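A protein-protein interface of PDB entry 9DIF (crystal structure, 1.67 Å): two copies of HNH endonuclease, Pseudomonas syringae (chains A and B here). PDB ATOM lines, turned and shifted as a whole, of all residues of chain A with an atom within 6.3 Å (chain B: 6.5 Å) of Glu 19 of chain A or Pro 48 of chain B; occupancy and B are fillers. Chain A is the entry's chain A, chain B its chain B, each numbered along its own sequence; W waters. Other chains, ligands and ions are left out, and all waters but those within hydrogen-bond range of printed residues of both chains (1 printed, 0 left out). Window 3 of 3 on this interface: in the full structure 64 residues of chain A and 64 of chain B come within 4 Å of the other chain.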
ATOM      1  N   ASN A  17      -1.395  23.012  28.430  1.00  0.00           N
ATOM      2  CA  ASN A  17      -0.509  23.496  29.487  1.00  0.00           C
ATOM      3  C   ASN A  17       0.878  23.876  28.933  1.00  0.00           C
ATOM      4  O   ASN A  17       1.218  23.657  27.756  1.00  0.00           O
ATOM      5  CB  ASN A  17      -0.376  22.457  30.609  1.00  0.00           C
ATOM      6  CG  ASN A  17       0.174  21.141  30.121  1.00  0.00           C
ATOM      7  OD1 ASN A  17       0.960  21.089  29.180  1.00  0.00           O
ATOM      8  ND2 ASN A  17      -0.259  20.065  30.741  1.00  0.00           N
ATOM      9  N   ASP A  18       1.675  24.481  29.810  1.00  0.00           N
ATOM     10  CA  ASP A  18       2.930  25.056  29.355  1.00  0.00           C
ATOM     11  C   ASP A  18       3.937  23.970  29.019  1.00  0.00           C
ATOM     12  O   ASP A  18       4.659  24.081  28.026  1.00  0.00           O
ATOM     13  CB  ASP A  18       3.454  26.029  30.411  1.00  0.00           C
ATOM     14  CG  ASP A  18       4.799  26.681  30.028  1.00  0.00           C
ATOM     15  OD1 ASP A  18       4.851  27.407  29.000  1.00  0.00           O
ATOM     16  OD2 ASP A  18       5.800  26.461  30.768  1.00  0.00           O
ATOM     17  N   GLU A  19       3.978  22.890  29.797  1.00  0.00           N
ATOM     18  CA  GLU A  19       4.875  21.785  29.470  1.00  0.00           C
ATOM     19  C   GLU A  19       4.623  21.245  28.061  1.00  0.00           C
ATOM     20  O   GLU A  19       5.567  20.852  27.360  1.00  0.00           O
ATOM     21  CB  GLU A  19       4.687  20.678  30.507  1.00  0.00           C
ATOM     22  CG  GLU A  19       5.385  19.375  30.166  1.00  0.00           C
ATOM     23  CD  GLU A  19       5.066  18.237  31.152  1.00  0.00           C
ATOM     24  OE1 GLU A  19       3.963  17.626  31.074  1.00  0.00           O
ATOM     25  OE2 GLU A  19       5.939  17.939  31.996  1.00  0.00           O
ATOM     26  N   THR A  20       3.362  21.167  27.645  1.00  0.00           N
ATOM     27  CA  THR A  20       3.064  20.578  26.337  1.00  0.00           C
ATOM     28  C   THR A  20       3.417  21.519  25.195  1.00  0.00           C
ATOM     29  O   THR A  20       3.948  21.090  24.159  1.00  0.00           O
ATOM     30  CB  THR A  20       1.595  20.221  26.259  1.00  0.00           C
ATOM     31  OG1 THR A  20       1.381  19.171  27.182  1.00  0.00           O
ATOM     32  CG2 THR A  20       1.256  19.728  24.921  1.00  0.00           C
ATOM     33  N   LYS A  21       3.140  22.802  25.375  1.00  0.00           N
ATOM     34  CA  LYS A  21       3.593  23.783  24.393  1.00  0.00           C
ATOM     35  C   LYS A  21       5.126  23.766  24.270  1.00  0.00           C
ATOM     36  O   LYS A  21       5.672  23.815  23.165  1.00  0.00           O
ATOM     37  CB  LYS A  21       3.048  25.160  24.773  1.00  0.00           C
ATOM     38  CG  LYS A  21       1.582  25.309  24.407  1.00  0.00           C
ATOM     39  CD  LYS A  21       0.840  26.295  25.297  1.00  0.00           C
ATOM     40  CE  LYS A  21       1.167  27.731  24.925  1.00  0.00           C
ATOM     41  NZ  LYS A  21      -0.058  28.610  25.097  1.00  0.00           N
ATOM     42  N   ARG A  22       5.824  23.648  25.384  1.00  0.00           N
ATOM     43  CA  ARG A  22       7.282  23.532  25.347  1.00  0.00           C
ATOM     44  C   ARG A  22       7.726  22.304  24.560  1.00  0.00           C
ATOM     45  O   ARG A  22       8.611  22.390  23.699  1.00  0.00           O
ATOM     46  CB  ARG A  22       7.758  23.482  26.797  1.00  0.00           C
ATOM     47  CG  ARG A  22       9.144  23.798  27.015  1.00  0.00           C
ATOM     48  CD  ARG A  22       9.358  24.355  28.499  1.00  0.00           C
ATOM     49  NE  ARG A  22      10.767  24.260  28.773  1.00  0.00           N
ATOM     50  CZ  ARG A  22      11.341  24.727  29.855  1.00  0.00           C
ATOM     51  NH1 ARG A  22      10.622  25.324  30.800  1.00  0.00           N
ATOM     52  NH2 ARG A  22      12.668  24.662  29.951  1.00  0.00           N
ATOM     53  N   ILE A  23       7.050  21.162  24.761  1.00  0.00           N
ATOM     54  CA  ILE A  23       7.304  19.971  23.934  1.00  0.00           C
ATOM     55  C   ILE A  23       7.025  20.215  22.445  1.00  0.00           C
ATOM     56  O   ILE A  23       7.804  19.777  21.572  1.00  0.00           O
ATOM     57  CB  ILE A  23       6.494  18.766  24.453  1.00  0.00           C
ATOM     58  CG1 ILE A  23       7.010  18.357  25.803  1.00  0.00           C
ATOM     59  CG2 ILE A  23       6.499  17.635  23.460  1.00  0.00           C
ATOM     60  CD1 ILE A  23       8.344  17.629  25.749  1.00  0.00           C
ATOM     61  N   VAL A  24       5.896  20.848  22.093  1.00  0.00           N
ATOM     62  CA  VAL A  24       5.609  21.119  20.688  1.00  0.00           C
ATOM     63  C   VAL A  24       6.724  21.944  20.073  1.00  0.00           C
ATOM     64  O   VAL A  24       7.153  21.697  18.950  1.00  0.00           O
ATOM     65  CB  VAL A  24       4.252  21.829  20.528  1.00  0.00           C
ATOM     66  CG1 VAL A  24       4.060  22.363  19.091  1.00  0.00           C
ATOM     67  CG2 VAL A  24       3.084  20.877  20.917  1.00  0.00           C
ATOM     68  N   ASP B  42      10.685  11.267  29.251  1.00  0.00           N
ATOM     69  CA  ASP B  42       9.779  11.354  30.392  1.00  0.00           C
ATOM     70  C   ASP B  42       8.397  11.785  29.955  1.00  0.00           C
ATOM     71  O   ASP B  42       7.399  11.221  30.404  1.00  0.00           O
ATOM     72  CB  ASP B  42      10.291  12.319  31.456  1.00  0.00           C
ATOM     73  CG  ASP B  42      11.343  11.689  32.387  1.00  0.00           C
ATOM     74  OD1 ASP B  42      11.580  10.460  32.246  1.00  0.00           O
ATOM     75  OD2 ASP B  42      11.930  12.405  33.256  1.00  0.00           O
ATOM     76  N   TYR B  43       8.318  12.818  29.109  1.00  0.00           N
ATOM     77  CA  TYR B  43       7.019  13.315  28.673  1.00  0.00           C
ATOM     78  C   TYR B  43       6.256  12.247  27.894  1.00  0.00           C
ATOM     79  O   TYR B  43       5.046  12.063  28.090  1.00  0.00           O
ATOM     80  CB  TYR B  43       7.185  14.584  27.826  1.00  0.00           C
ATOM     81  CG  TYR B  43       5.868  15.144  27.337  1.00  0.00           C
ATOM     82  CD1 TYR B  43       5.141  16.012  28.136  1.00  0.00           C
ATOM     83  CD2 TYR B  43       5.354  14.814  26.065  1.00  0.00           C
ATOM     84  CE1 TYR B  43       3.949  16.540  27.705  1.00  0.00           C
ATOM     85  CE2 TYR B  43       4.132  15.292  25.645  1.00  0.00           C
ATOM     86  CZ  TYR B  43       3.428  16.167  26.476  1.00  0.00           C
ATOM     87  OH  TYR B  43       2.200  16.678  26.066  1.00  0.00           O
ATOM     88  N   GLY B  46       4.368   9.904  30.089  1.00  0.00           N
ATOM     89  CA  GLY B  46       3.391  10.418  31.027  1.00  0.00           C
ATOM     90  C   GLY B  46       3.961  11.019  32.296  1.00  0.00           C
ATOM     91  O   GLY B  46       3.205  11.638  33.054  1.00  0.00           O
ATOM     92  N   LYS B  47       5.245  10.857  32.542  1.00  0.00           N
ATOM     93  CA  LYS B  47       5.949  11.443  33.659  1.00  0.00           C
ATOM     94  C   LYS B  47       6.240  12.929  33.394  1.00  0.00           C
ATOM     95  O   LYS B  47       6.478  13.347  32.249  1.00  0.00           O
ATOM     96  CB  LYS B  47       7.243  10.660  33.920  1.00  0.00           C
ATOM     97  CG  LYS B  47       8.369  11.460  34.580  1.00  0.00           C
ATOM     98  CD  LYS B  47       9.584  10.561  34.890  1.00  0.00           C
ATOM     99  CE  LYS B  47       9.337   9.706  36.152  1.00  0.00           C
ATOM    100  NZ  LYS B  47      10.579   9.029  36.609  1.00  0.00           N
ATOM    101  N   PRO B  48       6.209  13.751  34.436  1.00  0.00           N
ATOM    102  CA  PRO B  48       6.504  15.171  34.256  1.00  0.00           C
ATOM    103  C   PRO B  48       7.932  15.400  33.779  1.00  0.00           C
ATOM    104  O   PRO B  48       8.864  14.701  34.175  1.00  0.00           O
ATOM    105  CB  PRO B  48       6.286  15.756  35.660  1.00  0.00           C
ATOM    106  CG  PRO B  48       5.448  14.790  36.374  1.00  0.00           C
ATOM    107  CD  PRO B  48       5.866  13.447  35.832  1.00  0.00           C
ATOM    108  N   MET B  49       8.101  16.435  32.953  1.00  0.00           N
ATOM    109  CA  MET B  49       9.421  16.804  32.445  1.00  0.00           C
ATOM    110  C   MET B  49      10.207  17.603  33.483  1.00  0.00           C
ATOM    111  O   MET B  49       9.703  18.589  34.028  1.00  0.00           O
ATOM    112  CB  MET B  49       9.296  17.632  31.161  1.00  0.00           C
ATOM    113  CG  MET B  49       9.119  16.850  29.913  1.00  0.00           C
ATOM    114  SD  MET B  49      10.533  15.799  29.598  1.00  0.00           S
ATOM    115  CE  MET B  49      11.739  16.951  28.976  1.00  0.00           C
ATOM    116  N   LYS B  50      11.437  17.169  33.761  1.00  0.00           N
ATOM    117  CA  LYS B  50      12.364  17.863  34.645  1.00  0.00           C
ATOM    118  C   LYS B  50      13.487  18.316  33.729  1.00  0.00           C
ATOM    119  O   LYS B  50      14.571  17.743  33.726  1.00  0.00           O
ATOM    120  CB  LYS B  50      12.868  16.978  35.742  1.00  0.00           C
ATOM    121  CG  LYS B  50      11.732  16.388  36.557  1.00  0.00           C
ATOM    122  CD  LYS B  50      12.201  15.695  37.831  1.00  0.00           C
ATOM    123  CE  LYS B  50      12.550  16.708  38.928  1.00  0.00           C
ATOM    124  NZ  LYS B  50      12.967  16.021  40.208  1.00  0.00           N
ATOM    125  N   TRP B  51      13.206  19.375  32.961  1.00  0.00           N
ATOM    126  CA  TRP B  51      14.081  19.829  31.886  1.00  0.00           C
ATOM    127  C   TRP B  51      15.517  20.003  32.347  1.00  0.00           C
ATOM    128  O   TRP B  51      16.448  19.652  31.620  1.00  0.00           O
ATOM    129  CB  TRP B  51      13.570  21.164  31.319  1.00  0.00           C
ATOM    130  CG  TRP B  51      12.142  21.133  30.905  1.00  0.00           C
ATOM    131  CD1 TRP B  51      11.074  21.465  31.663  1.00  0.00           C
ATOM    132  CD2 TRP B  51      11.626  20.758  29.611  1.00  0.00           C
ATOM    133  NE1 TRP B  51       9.907  21.305  30.933  1.00  0.00           N
ATOM    134  CE2 TRP B  51      10.219  20.859  29.677  1.00  0.00           C
ATOM    135  CE3 TRP B  51      12.213  20.372  28.407  1.00  0.00           C
ATOM    136  CZ2 TRP B  51       9.396  20.561  28.600  1.00  0.00           C
ATOM    137  CZ3 TRP B  51      11.399  20.059  27.346  1.00  0.00           C
ATOM    138  CH2 TRP B  51       9.998  20.171  27.446  1.00  0.00           C
HETATM  139  O   HOH W   1       6.990  20.149  33.577  1.00  0.00           O
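N of Met 49 of chain B lies within hydrogen-bond range of OE2 of Glu 19 of chain A.
The side-chain hydroxyl (OG1) of Thr 20 of chain A is in hydrogen-bond range of the side-chain hydroxyl (OH) of Tyr 43 of chain B, at 2.9 Å.
Of the 8 printed residues of chain A, 4 touch a printed residue of chain B.
Along chain A the printed residues that touch a printed residue of chain B span positions 19 to 23.
Among the printed residues, 7 pairs touch across the chains.
Among the printed residues, no Asp or Glu carboxylate lies within 4 Å of a Lys or Arg side-chain nitrogen of the other chain.
Glu 19 of chain A touches Tyr 43 of chain B.
Pro 48 of chain B touches Glu 19 of chain A (CA to OE2, 3.6 Å).
CE2 of Trp 51 of chain B touches NE of Arg 22 of chain A, at 3.6 Å.
CG1 of Ile 23 of chain A touches CG of Tyr 43 of chain B (3.7 Å).
Ile 23 of chain A touches Trp 51 of chain B.
Of chain B, only Tyr 43, Pro 48 and Met 49 come within 4 Å of Glu 19 of chain A.
Of chain A, only Glu 19 comes within 4 Å of Pro 48 of chain B.
Of the printed residues of chain A, Met 49 of chain B touches Glu 19 (2.8 Å).
Of the printed residues of chain B, Ile 23 of chain A touches Tyr 43 and Trp 51.
Of the printed residues of chain A, Trp 51 of chain B touches Arg 22 and Ile 23.
The nearest residue of chain B that does not touch Glu 19 of chain A is Trp 51 of chain B (4.04 Å).
The nearest printed residue of chain A that does not touch Pro 48 of chain B is Ile 23 of chain A (8.3 Å).
No position is printed for both chains.
Of the 7 pairs that touch across the chains among the printed residues, none has its exchanged pair printed and touching as well.
Water W1 lies within hydrogen-bond range of the side-chain carboxylate of Glu 19 of chain A (2.9 Å) and the backbone carbonyl oxygen of Met 49 of chain B (3.2 Å).
The side-chain hydroxyl (OG1) of Thr 20 of chain A lies within hydrogen-bond range of the side-chain amide oxygen (OD1) of Asn 17 of chain A.
The backbone NH (N) of Tyr 43 of chain B sits at hydrogen-bond distance from the side-chain sulfur (SD) of Met 49 of chain B (3.7 Å).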
